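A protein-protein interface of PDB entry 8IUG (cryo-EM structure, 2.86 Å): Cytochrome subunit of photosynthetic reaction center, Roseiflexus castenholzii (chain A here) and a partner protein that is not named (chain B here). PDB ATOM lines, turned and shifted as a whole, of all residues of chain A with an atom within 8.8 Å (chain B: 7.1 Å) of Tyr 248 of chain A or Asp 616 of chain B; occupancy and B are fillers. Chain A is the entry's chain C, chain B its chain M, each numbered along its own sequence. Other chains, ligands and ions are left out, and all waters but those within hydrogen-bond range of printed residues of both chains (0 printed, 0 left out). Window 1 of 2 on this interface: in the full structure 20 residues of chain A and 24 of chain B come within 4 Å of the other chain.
His 515 of chain B touches Val 211 of chain A (CD2 to O, 3.1 Å). O of His 515 of chain B touches CA of Thr 212 of chain A (3.4 Å). Gly 517 of chain B touches Thr 212 of chain A. Thr 212 of chain A touches Asp 616 of chain B (CG2 to OD2, 3.3 Å). CA of Gly 213 of chain A touches O of Pro 615 of chain B (3.4 Å). CE of Lys 215 of chain A touches O of Gly 611 of chain B, 3.6 Å away. Tyr 618 of chain B touches Arg 247 of chain A. Asp 616 of chain B touches Tyr 248 of chain A (OD2 to OH, 3.5 Å). Tyr 618 of chain B touches Tyr 248 of chain A.
Of the 17 printed residues of chain B, 7 touch a printed residue of chain A. Hydrophobic or aromatic side chains of chain B that line the printed part of chain A: His 515 and Tyr 618.
Printed residues of chain B within 4 Å of Lys 215 of chain A: Gly 611. Of the printed residues of chain B, Arg 247 of chain A touches Asn 518 and Tyr 618. Of chain B, only Asp 616 and Tyr 618 come within 4 Å of Tyr 248 of chain A. Phe 249 of chain A touches none of the printed residues of chain B. Printed residues of chain A within 4 Å of Gly 517 of chain B: Thr 212. Printed residues of chain A within 4 Å of Asn 518 of chain B: Arg 247 (3.3 Å). Asp 616 of chain B touches two residues of chain A. Of the printed residues of chain A, Tyr 618 of chain B touches Arg 247 (3.6 Å) and Tyr 248 (3.5 Å). The nearest printed residue of chain B that does not touch Arg 214 of chain A is Trp 516 of chain B (4.1 Å).
The backbone NH (N) of Gly 213 of chain A sits at hydrogen-bond distance from the backbone carbonyl oxygen (O) of His 515 of chain B (3.1 Å). A ring nitrogen (NE2) of His 515 of chain B lies within hydrogen-bond range of the backbone carbonyl oxygen (O) of Arg 214 of chain A, at 2.8 Å. O of Arg 247 of chain A is in hydrogen-bond range of ND2 of Asn 518 of chain B (3.3 Å).
The backbone NH (N) of Arg 247 of chain A lies close to the side-chain amide oxygen (OD1) of Asn 245 of chain A (3.5 Å). The side-chain carboxylate (OD1) of Asp 616 of chain B is in hydrogen-bond range of the backbone NH (N) of Tyr 618 of chain B (3.4 Å). OD1 of Asp 616 of chain B is in hydrogen-bond range of N of Ala 619 of chain B (3.2 Å).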
ATOM      1  N   VAL A 211      23.329  -2.856  16.237  1.00  0.00           N
ATOM      2  CA  VAL A 211      23.808  -2.545  14.893  1.00  0.00           C
ATOM      3  C   VAL A 211      25.093  -1.736  14.876  1.00  0.00           C
ATOM      4  O   VAL A 211      25.741  -1.649  13.820  1.00  0.00           O
ATOM      5  CB  VAL A 211      22.711  -1.811  14.080  1.00  0.00           C
ATOM      6  CG1 VAL A 211      21.467  -2.664  13.938  1.00  0.00           C
ATOM      7  CG2 VAL A 211      22.375  -0.472  14.714  1.00  0.00           C
ATOM      8  N   THR A 212      25.522  -1.133  15.982  1.00  0.00           N
ATOM      9  CA  THR A 212      26.611  -0.163  15.941  1.00  0.00           C
ATOM     10  C   THR A 212      27.955  -0.859  15.760  1.00  0.00           C
ATOM     11  O   THR A 212      28.323  -1.733  16.551  1.00  0.00           O
ATOM     12  CB  THR A 212      26.619   0.679  17.213  1.00  0.00           C
ATOM     13  OG1 THR A 212      25.460   1.516  17.241  1.00  0.00           O
ATOM     14  CG2 THR A 212      27.850   1.551  17.261  1.00  0.00           C
ATOM     15  N   GLY A 213      28.689  -0.462  14.721  1.00  0.00           N
ATOM     16  CA  GLY A 213      30.027  -0.961  14.488  1.00  0.00           C
ATOM     17  C   GLY A 213      30.118  -2.313  13.822  1.00  0.00           C
ATOM     18  O   GLY A 213      31.223  -2.847  13.699  1.00  0.00           O
ATOM     19  N   ARG A 214      29.001  -2.881  13.379  1.00  0.00           N
ATOM     20  CA  ARG A 214      28.988  -4.227  12.826  1.00  0.00           C
ATOM     21  C   ARG A 214      29.161  -4.179  11.315  1.00  0.00           C
ATOM     22  O   ARG A 214      28.396  -3.510  10.616  1.00  0.00           O
ATOM     23  CB  ARG A 214      27.689  -4.942  13.187  1.00  0.00           C
ATOM     24  CG  ARG A 214      27.550  -5.237  14.658  1.00  0.00           C
ATOM     25  CD  ARG A 214      27.076  -6.650  14.875  1.00  0.00           C
ATOM     26  NE  ARG A 214      25.651  -6.793  14.623  1.00  0.00           N
ATOM     27  CZ  ARG A 214      25.045  -7.946  14.386  1.00  0.00           C
ATOM     28  NH1 ARG A 214      25.724  -9.077  14.299  1.00  0.00           N
ATOM     29  NH2 ARG A 214      23.727  -7.965  14.229  1.00  0.00           N
ATOM     30  N   LYS A 215      30.165  -4.893  10.819  1.00  0.00           N
ATOM     31  CA  LYS A 215      30.459  -4.953   9.396  1.00  0.00           C
ATOM     32  C   LYS A 215      29.792  -6.131   8.704  1.00  0.00           C
ATOM     33  O   LYS A 215      29.958  -6.295   7.492  1.00  0.00           O
ATOM     34  CB  LYS A 215      31.971  -5.001   9.176  1.00  0.00           C
ATOM     35  CG  LYS A 215      32.680  -3.720   9.565  1.00  0.00           C
ATOM     36  CD  LYS A 215      34.149  -3.768   9.209  1.00  0.00           C
ATOM     37  CE  LYS A 215      34.845  -2.475   9.587  1.00  0.00           C
ATOM     38  NZ  LYS A 215      36.318  -2.548   9.384  1.00  0.00           N
ATOM     39  N   CYS A 243      14.930   6.092  27.164  1.00  0.00           N
ATOM     40  CA  CYS A 243      15.807   4.918  27.363  1.00  0.00           C
ATOM     41  C   CYS A 243      17.258   5.191  26.884  1.00  0.00           C
ATOM     42  O   CYS A 243      18.099   4.429  27.332  1.00  0.00           O
ATOM     43  CB  CYS A 243      15.204   3.675  26.714  1.00  0.00           C
ATOM     44  SG  CYS A 243      13.489   3.137  27.048  1.00  0.00           S
ATOM     45  N   HIS A 244      17.585   6.229  26.069  1.00  0.00           N
ATOM     46  CA  HIS A 244      18.942   6.420  25.581  1.00  0.00           C
ATOM     47  C   HIS A 244      19.468   7.810  25.889  1.00  0.00           C
ATOM     48  O   HIS A 244      18.710   8.770  26.026  1.00  0.00           O
ATOM     49  CB  HIS A 244      19.030   6.227  24.065  1.00  0.00           C
ATOM     50  CG  HIS A 244      18.659   4.857  23.602  1.00  0.00           C
ATOM     51  ND1 HIS A 244      19.534   3.797  23.641  1.00  0.00           N
ATOM     52  CD2 HIS A 244      17.507   4.377  23.086  1.00  0.00           C
ATOM     53  CE1 HIS A 244      18.936   2.721  23.169  1.00  0.00           C
ATOM     54  NE2 HIS A 244      17.704   3.045  22.827  1.00  0.00           N
ATOM     55  N   ASN A 245      20.791   7.894  25.989  1.00  0.00           N
ATOM     56  CA  ASN A 245      21.533   9.125  25.750  1.00  0.00           C
ATOM     57  C   ASN A 245      21.856   9.137  24.259  1.00  0.00           C
ATOM     58  O   ASN A 245      22.596   8.280  23.773  1.00  0.00           O
ATOM     59  CB  ASN A 245      22.795   9.172  26.606  1.00  0.00           C
ATOM     60  CG  ASN A 245      23.436  10.543  26.640  1.00  0.00           C
ATOM     61  OD1 ASN A 245      23.322  11.316  25.698  1.00  0.00           O
ATOM     62  ND2 ASN A 245      24.120  10.847  27.729  1.00  0.00           N
ATOM     63  N   ALA A 246      21.286  10.095  23.531  1.00  0.00           N
ATOM     64  CA  ALA A 246      21.298  10.037  22.077  1.00  0.00           C
ATOM     65  C   ALA A 246      22.668  10.304  21.473  1.00  0.00           C
ATOM     66  O   ALA A 246      22.816  10.164  20.257  1.00  0.00           O
ATOM     67  CB  ALA A 246      20.282  11.021  21.511  1.00  0.00           C
ATOM     68  N   ARG A 247      23.659  10.695  22.271  1.00  0.00           N
ATOM     69  CA  ARG A 247      25.018  10.825  21.765  1.00  0.00           C
ATOM     70  C   ARG A 247      25.746   9.489  21.696  1.00  0.00           C
ATOM     71  O   ARG A 247      26.809   9.415  21.076  1.00  0.00           O
ATOM     72  CB  ARG A 247      25.816  11.813  22.620  1.00  0.00           C
ATOM     73  CG  ARG A 247      26.437  11.235  23.872  1.00  0.00           C
ATOM     74  CD  ARG A 247      27.325  12.261  24.554  1.00  0.00           C
ATOM     75  NE  ARG A 247      28.017  11.719  25.715  1.00  0.00           N
ATOM     76  CZ  ARG A 247      28.895  12.389  26.447  1.00  0.00           C
ATOM     77  NH1 ARG A 247      29.204  13.644  26.178  1.00  0.00           N
ATOM     78  NH2 ARG A 247      29.480  11.784  27.473  1.00  0.00           N
ATOM     79  N   TYR A 248      25.201   8.443  22.316  1.00  0.00           N
ATOM     80  CA  TYR A 248      25.731   7.089  22.170  1.00  0.00           C
ATOM     81  C   TYR A 248      24.608   6.121  22.521  1.00  0.00           C
ATOM     82  O   TYR A 248      24.258   5.984  23.695  1.00  0.00           O
ATOM     83  CB  TYR A 248      26.944   6.885  23.062  1.00  0.00           C
ATOM     84  CG  TYR A 248      27.805   5.700  22.690  1.00  0.00           C
ATOM     85  CD1 TYR A 248      28.230   5.505  21.385  1.00  0.00           C
ATOM     86  CD2 TYR A 248      28.211   4.790  23.650  1.00  0.00           C
ATOM     87  CE1 TYR A 248      29.018   4.431  21.047  1.00  0.00           C
ATOM     88  CE2 TYR A 248      28.999   3.717  23.320  1.00  0.00           C
ATOM     89  CZ  TYR A 248      29.399   3.541  22.019  1.00  0.00           C
ATOM     90  OH  TYR A 248      30.188   2.465  21.698  1.00  0.00           O
ATOM     91  N   PHE A 249      24.040   5.470  21.513  1.00  0.00           N
ATOM     92  CA  PHE A 249      22.928   4.544  21.698  1.00  0.00           C
ATOM     93  C   PHE A 249      23.306   3.220  22.364  1.00  0.00           C
ATOM     94  O   PHE A 249      22.448   2.615  23.016  1.00  0.00           O
ATOM     95  CB  PHE A 249      22.231   4.284  20.364  1.00  0.00           C
ATOM     96  CG  PHE A 249      21.386   5.429  19.903  1.00  0.00           C
ATOM     97  CD1 PHE A 249      20.301   5.841  20.639  1.00  0.00           C
ATOM     98  CD2 PHE A 249      21.680   6.101  18.739  1.00  0.00           C
ATOM     99  CE1 PHE A 249      19.530   6.890  20.223  1.00  0.00           C
ATOM    100  CE2 PHE A 249      20.909   7.153  18.323  1.00  0.00           C
ATOM    101  CZ  PHE A 249      19.837   7.545  19.067  1.00  0.00           C
ATOM    102  N   PRO A 250      24.530   2.703  22.199  1.00  0.00           N
ATOM    103  CA  PRO A 250      24.926   1.519  22.981  1.00  0.00           C
ATOM    104  C   PRO A 250      24.992   1.733  24.488  1.00  0.00           C
ATOM    105  O   PRO A 250      25.054   0.745  25.226  1.00  0.00           O
ATOM    106  CB  PRO A 250      26.306   1.183  22.411  1.00  0.00           C
ATOM    107  CG  PRO A 250      26.219   1.609  21.027  1.00  0.00           C
ATOM    108  CD  PRO A 250      25.413   2.865  21.030  1.00  0.00           C
ATOM    109  N   SER A 251      24.984   2.972  24.969  1.00  0.00           N
ATOM    110  CA  SER A 251      25.178   3.236  26.390  1.00  0.00           C
ATOM    111  C   SER A 251      23.998   2.748  27.223  1.00  0.00           C
ATOM    112  O   SER A 251      22.837   2.891  26.834  1.00  0.00           O
ATOM    113  CB  SER A 251      25.391   4.730  26.611  1.00  0.00           C
ATOM    114  OG  SER A 251      25.723   5.009  27.955  1.00  0.00           O
ATOM    115  N   TYR A 252      24.301   2.193  28.395  1.00  0.00           N
ATOM    116  CA  TYR A 252      23.308   1.669  29.328  1.00  0.00           C
ATOM    117  C   TYR A 252      23.179   2.546  30.570  1.00  0.00           C
ATOM    118  O   TYR A 252      23.004   2.046  31.679  1.00  0.00           O
ATOM    119  CB  TYR A 252      23.655   0.244  29.744  1.00  0.00           C
ATOM    120  CG  TYR A 252      23.000  -0.835  28.922  1.00  0.00           C
ATOM    121  CD1 TYR A 252      21.715  -1.260  29.205  1.00  0.00           C
ATOM    122  CD2 TYR A 252      23.672  -1.435  27.874  1.00  0.00           C
ATOM    123  CE1 TYR A 252      21.114  -2.244  28.460  1.00  0.00           C
ATOM    124  CE2 TYR A 252      23.080  -2.419  27.126  1.00  0.00           C
ATOM    125  CZ  TYR A 252      21.801  -2.820  27.421  1.00  0.00           C
ATOM    126  OH  TYR A 252      21.209  -3.806  26.671  1.00  0.00           O
ATOM    127  N   GLU A 253      23.253   3.861  30.402  1.00  0.00           N
ATOM    128  CA  GLU A 253      23.295   4.775  31.534  1.00  0.00           C
ATOM    129  C   GLU A 253      21.919   5.245  31.991  1.00  0.00           C
ATOM    130  O   GLU A 253      21.836   6.029  32.941  1.00  0.00           O
ATOM    131  CB  GLU A 253      24.166   5.983  31.195  1.00  0.00           C
ATOM    132  CG  GLU A 253      24.026   6.467  29.775  1.00  0.00           C
ATOM    133  CD  GLU A 253      24.619   7.838  29.583  1.00  0.00           C
ATOM    134  OE1 GLU A 253      24.155   8.786  30.246  1.00  0.00           O
ATOM    135  OE2 GLU A 253      25.562   7.969  28.782  1.00  0.00           O
ATOM    136  N   ILE A 254      20.845   4.790  31.350  1.00  0.00           N
ATOM    137  CA  ILE A 254      19.480   5.022  31.804  1.00  0.00           C
ATOM    138  C   ILE A 254      18.900   3.680  32.228  1.00  0.00           C
ATOM    139  O   ILE A 254      19.124   2.663  31.561  1.00  0.00           O
ATOM    140  CB  ILE A 254      18.616   5.676  30.705  1.00  0.00           C
ATOM    141  CG1 ILE A 254      19.415   6.728  29.928  1.00  0.00           C
ATOM    142  CG2 ILE A 254      17.372   6.296  31.299  1.00  0.00           C
ATOM    143  CD1 ILE A 254      19.511   8.069  30.583  1.00  0.00           C
ATOM    144  N   LYS A 257      16.459   1.269  30.035  1.00  0.00           N
ATOM    145  CA  LYS A 257      16.969   0.301  29.067  1.00  0.00           C
ATOM    146  C   LYS A 257      17.038  -1.103  29.664  1.00  0.00           C
ATOM    147  O   LYS A 257      16.691  -2.087  28.997  1.00  0.00           O
ATOM    148  CB  LYS A 257      18.341   0.743  28.560  1.00  0.00           C
ATOM    149  CG  LYS A 257      18.531   0.598  27.059  1.00  0.00           C
ATOM    150  CD  LYS A 257      19.990   0.679  26.672  1.00  0.00           C
ATOM    151  CE  LYS A 257      20.179   0.356  25.212  1.00  0.00           C
ATOM    152  NZ  LYS A 257      21.584   0.139  24.825  1.00  0.00           N
ATOM    153  N   HIS B 515      24.557   3.762  12.222  1.00  0.00           N
ATOM    154  CA  HIS B 515      25.338   2.540  12.058  1.00  0.00           C
ATOM    155  C   HIS B 515      26.775   2.722  12.531  1.00  0.00           C
ATOM    156  O   HIS B 515      27.310   1.879  13.257  1.00  0.00           O
ATOM    157  CB  HIS B 515      25.301   2.121  10.589  1.00  0.00           C
ATOM    158  CG  HIS B 515      25.831   0.746  10.323  1.00  0.00           C
ATOM    159  ND1 HIS B 515      25.873   0.206   9.058  1.00  0.00           N
ATOM    160  CD2 HIS B 515      26.336  -0.197  11.151  1.00  0.00           C
ATOM    161  CE1 HIS B 515      26.384  -1.008   9.117  1.00  0.00           C
ATOM    162  NE2 HIS B 515      26.672  -1.279  10.375  1.00  0.00           N
ATOM    163  N   TRP B 516      27.425   3.800  12.111  1.00  0.00           N
ATOM    164  CA  TRP B 516      28.841   4.018  12.409  1.00  0.00           C
ATOM    165  C   TRP B 516      29.022   4.985  13.577  1.00  0.00           C
ATOM    166  O   TRP B 516      29.597   6.056  13.439  1.00  0.00           O
ATOM    167  CB  TRP B 516      29.568   4.522  11.168  1.00  0.00           C
ATOM    168  CG  TRP B 516      29.367   3.670   9.966  1.00  0.00           C
ATOM    169  CD1 TRP B 516      28.796   4.040   8.791  1.00  0.00           C
ATOM    170  CD2 TRP B 516      29.727   2.294   9.822  1.00  0.00           C
ATOM    171  NE1 TRP B 516      28.783   2.985   7.919  1.00  0.00           N
ATOM    172  CE2 TRP B 516      29.350   1.899   8.529  1.00  0.00           C
ATOM    173  CE3 TRP B 516      30.335   1.357  10.661  1.00  0.00           C
ATOM    174  CZ2 TRP B 516      29.560   0.613   8.057  1.00  0.00           C
ATOM    175  CZ3 TRP B 516      30.539   0.087  10.192  1.00  0.00           C
ATOM    176  CH2 TRP B 516      30.155  -0.277   8.903  1.00  0.00           C
ATOM    177  N   GLY B 517      28.550   4.577  14.749  1.00  0.00           N
ATOM    178  CA  GLY B 517      28.708   5.417  15.926  1.00  0.00           C
ATOM    179  C   GLY B 517      27.850   6.660  15.830  1.00  0.00           C
ATOM    180  O   GLY B 517      26.663   6.597  15.503  1.00  0.00           O
ATOM    181  N   ASN B 518      28.445   7.808  16.125  1.00  0.00           N
ATOM    182  CA  ASN B 518      27.769   9.095  16.051  1.00  0.00           C
ATOM    183  C   ASN B 518      28.526   9.975  15.070  1.00  0.00           C
ATOM    184  O   ASN B 518      29.738  10.150  15.204  1.00  0.00           O
ATOM    185  CB  ASN B 518      27.705   9.742  17.438  1.00  0.00           C
ATOM    186  CG  ASN B 518      26.819  10.958  17.487  1.00  0.00           C
ATOM    187  OD1 ASN B 518      26.101  11.258  16.542  1.00  0.00           O
ATOM    188  ND2 ASN B 518      26.860  11.665  18.600  1.00  0.00           N
ATOM    189  N   TYR B 521      30.880  13.231  15.897  1.00  0.00           N
ATOM    190  CA  TYR B 521      32.281  13.068  16.255  1.00  0.00           C
ATOM    191  C   TYR B 521      33.144  12.638  15.076  1.00  0.00           C
ATOM    192  O   TYR B 521      34.234  12.099  15.278  1.00  0.00           O
ATOM    193  CB  TYR B 521      32.405  12.085  17.417  1.00  0.00           C
ATOM    194  CG  TYR B 521      31.815  12.649  18.683  1.00  0.00           C
ATOM    195  CD1 TYR B 521      32.489  13.625  19.405  1.00  0.00           C
ATOM    196  CD2 TYR B 521      30.573  12.242  19.136  1.00  0.00           C
ATOM    197  CE1 TYR B 521      31.951  14.163  20.543  1.00  0.00           C
ATOM    198  CE2 TYR B 521      30.029  12.778  20.283  1.00  0.00           C
ATOM    199  CZ  TYR B 521      30.723  13.737  20.980  1.00  0.00           C
ATOM    200  OH  TYR B 521      30.193  14.277  22.124  1.00  0.00           O
ATOM    201  N   SER B 610      34.178   6.672   6.837  1.00  0.00           N
ATOM    202  CA  SER B 610      33.204   6.386   7.889  1.00  0.00           C
ATOM    203  C   SER B 610      33.089   4.898   8.208  1.00  0.00           C
ATOM    204  O   SER B 610      33.040   4.518   9.379  1.00  0.00           O
ATOM    205  CB  SER B 610      31.844   6.951   7.497  1.00  0.00           C
ATOM    206  OG  SER B 610      30.890   6.699   8.503  1.00  0.00           O
ATOM    207  N   GLY B 611      33.025   4.041   7.204  1.00  0.00           N
ATOM    208  CA  GLY B 611      32.794   2.647   7.519  1.00  0.00           C
ATOM    209  C   GLY B 611      34.015   1.756   7.447  1.00  0.00           C
ATOM    210  O   GLY B 611      34.083   0.722   8.113  1.00  0.00           O
ATOM    211  N   LEU B 613      37.513   2.481   7.877  1.00  0.00           N
ATOM    212  CA  LEU B 613      38.636   2.599   8.801  1.00  0.00           C
ATOM    213  C   LEU B 613      38.218   2.813  10.245  1.00  0.00           C
ATOM    214  O   LEU B 613      38.826   2.230  11.143  1.00  0.00           O
ATOM    215  CB  LEU B 613      39.566   3.743   8.373  1.00  0.00           C
ATOM    216  CG  LEU B 613      40.375   3.555   7.090  1.00  0.00           C
ATOM    217  CD1 LEU B 613      41.245   4.760   6.848  1.00  0.00           C
ATOM    218  CD2 LEU B 613      41.221   2.302   7.159  1.00  0.00           C
ATOM    219  N   VAL B 614      37.203   3.628  10.499  1.00  0.00           N
ATOM    220  CA  VAL B 614      36.734   3.911  11.848  1.00  0.00           C
ATOM    221  C   VAL B 614      35.286   3.447  11.962  1.00  0.00           C
ATOM    222  O   VAL B 614      34.360   4.176  11.612  1.00  0.00           O
ATOM    223  CB  VAL B 614      36.866   5.404  12.193  1.00  0.00           C
ATOM    224  CG1 VAL B 614      36.388   5.660  13.605  1.00  0.00           C
ATOM    225  CG2 VAL B 614      38.302   5.855  12.033  1.00  0.00           C
ATOM    226  N   PRO B 615      35.050   2.241  12.489  1.00  0.00           N
ATOM    227  CA  PRO B 615      33.680   1.716  12.568  1.00  0.00           C
ATOM    228  C   PRO B 615      32.822   2.342  13.655  1.00  0.00           C
ATOM    229  O   PRO B 615      31.662   1.947  13.803  1.00  0.00           O
ATOM    230  CB  PRO B 615      33.909   0.229  12.852  1.00  0.00           C
ATOM    231  CG  PRO B 615      35.171   0.210  13.616  1.00  0.00           C
ATOM    232  CD  PRO B 615      36.031   1.286  13.026  1.00  0.00           C
ATOM    233  N   ASP B 616      33.346   3.288  14.426  1.00  0.00           N
ATOM    234  CA  ASP B 616      32.619   3.860  15.554  1.00  0.00           C
ATOM    235  C   ASP B 616      33.287   5.179  15.898  1.00  0.00           C
ATOM    236  O   ASP B 616      34.452   5.188  16.300  1.00  0.00           O
ATOM    237  CB  ASP B 616      32.639   2.900  16.740  1.00  0.00           C
ATOM    238  CG  ASP B 616      31.656   3.274  17.819  1.00  0.00           C
ATOM    239  OD1 ASP B 616      31.668   4.431  18.268  1.00  0.00           O
ATOM    240  OD2 ASP B 616      30.869   2.401  18.228  1.00  0.00           O
ATOM    241  N   TRP B 617      32.566   6.283  15.740  1.00  0.00           N
ATOM    242  CA  TRP B 617      33.181   7.596  15.872  1.00  0.00           C
ATOM    243  C   TRP B 617      33.168   8.130  17.295  1.00  0.00           C
ATOM    244  O   TRP B 617      34.068   8.889  17.665  1.00  0.00           O
ATOM    245  CB  TRP B 617      32.499   8.591  14.933  1.00  0.00           C
ATOM    246  CG  TRP B 617      32.870   8.396  13.493  1.00  0.00           C
ATOM    247  CD1 TRP B 617      32.076   7.911  12.502  1.00  0.00           C
ATOM    248  CD2 TRP B 617      34.142   8.667  12.891  1.00  0.00           C
ATOM    249  NE1 TRP B 617      32.767   7.868  11.320  1.00  0.00           N
ATOM    250  CE2 TRP B 617      34.038   8.328  11.531  1.00  0.00           C
ATOM    251  CE3 TRP B 617      35.357   9.168  13.369  1.00  0.00           C
ATOM    252  CZ2 TRP B 617      35.098   8.475  10.645  1.00  0.00           C
ATOM    253  CZ3 TRP B 617      36.401   9.314  12.492  1.00  0.00           C
ATOM    254  CH2 TRP B 617      36.267   8.970  11.144  1.00  0.00           C
ATOM    255  N   TYR B 618      32.179   7.756  18.108  1.00  0.00           N
ATOM    256  CA  TYR B 618      32.174   8.188  19.503  1.00  0.00           C
ATOM    257  C   TYR B 618      33.307   7.538  20.289  1.00  0.00           C
ATOM    258  O   TYR B 618      33.983   8.205  21.081  1.00  0.00           O
ATOM    259  CB  TYR B 618      30.820   7.881  20.139  1.00  0.00           C
ATOM    260  CG  TYR B 618      30.743   8.157  21.625  1.00  0.00           C
ATOM    261  CD1 TYR B 618      30.361   9.398  22.104  1.00  0.00           C
ATOM    262  CD2 TYR B 618      31.041   7.167  22.548  1.00  0.00           C
ATOM    263  CE1 TYR B 618      30.288   9.642  23.453  1.00  0.00           C
ATOM    264  CE2 TYR B 618      30.972   7.404  23.891  1.00  0.00           C
ATOM    265  CZ  TYR B 618      30.594   8.639  24.340  1.00  0.00           C
ATOM    266  OH  TYR B 618      30.529   8.862  25.689  1.00  0.00           O
ATOM    267  N   ALA B 619      33.533   6.239  20.083  1.00  0.00           N
ATOM    268  CA  ALA B 619      34.643   5.564  20.748  1.00  0.00           C
ATOM    269  C   ALA B 619      35.986   6.118  20.290  1.00  0.00           C
ATOM    270  O   ALA B 619      36.903   6.307  21.101  1.00  0.00           O
ATOM    271  CB  ALA B 619      34.562   4.063  20.491  1.00  0.00           C
ATOM    272  N   TRP B 620      36.121   6.384  18.990  1.00  0.00           N
ATOM    273  CA  TRP B 620      37.340   7.003  18.482  1.00  0.00           C
ATOM    274  C   TRP B 620      37.565   8.370  19.114  1.00  0.00           C
ATOM    275  O   TRP B 620      38.681   8.693  19.527  1.00  0.00           O
ATOM    276  CB  TRP B 620      37.274   7.113  16.959  1.00  0.00           C
ATOM    277  CG  TRP B 620      38.434   7.833  16.359  1.00  0.00           C
ATOM    278  CD1 TRP B 620      39.601   7.284  15.932  1.00  0.00           C
ATOM    279  CD2 TRP B 620      38.543   9.240  16.121  1.00  0.00           C
ATOM    280  NE1 TRP B 620      40.431   8.258  15.445  1.00  0.00           N
ATOM    281  CE2 TRP B 620      39.804   9.470  15.553  1.00  0.00           C
ATOM    282  CE3 TRP B 620      37.694  10.330  16.337  1.00  0.00           C
ATOM    283  CZ2 TRP B 620      40.237  10.738  15.197  1.00  0.00           C
ATOM    284  CZ3 TRP B 620      38.129  11.585  15.988  1.00  0.00           C
ATOM    285  CH2 TRP B 620      39.386  11.781  15.423  1.00  0.00           C
ATOM    286  N   GLY B 621      36.515   9.187  19.202  1.00  0.00           N
ATOM    287  CA  GLY B 621      36.648  10.482  19.842  1.00  0.00           C
ATOM    288  C   GLY B 621      37.008  10.378  21.307  1.00  0.00           C
ATOM    289  O   GLY B 621      37.693  11.247  21.844  1.00  0.00           O
ATOM    290  N   GLU B 622      36.538   9.328  21.977  1.00  0.00           N
ATOM    291  CA  GLU B 622      36.966   9.085  23.350  1.00  0.00           C
ATOM    292  C   GLU B 622      38.457   8.786  23.424  1.00  0.00           C
ATOM    293  O   GLU B 622      39.153   9.295  24.308  1.00  0.00           O
ATOM    294  CB  GLU B 622      36.165   7.939  23.956  1.00  0.00           C
ATOM    295  CG  GLU B 622      34.819   8.348  24.473  1.00  0.00           C
ATOM    296  CD  GLU B 622      34.342   7.448  25.579  1.00  0.00           C
ATOM    297  OE1 GLU B 622      34.107   6.253  25.310  1.00  0.00           O
ATOM    298  OE2 GLU B 622      34.189   7.934  26.717  1.00  0.00           O
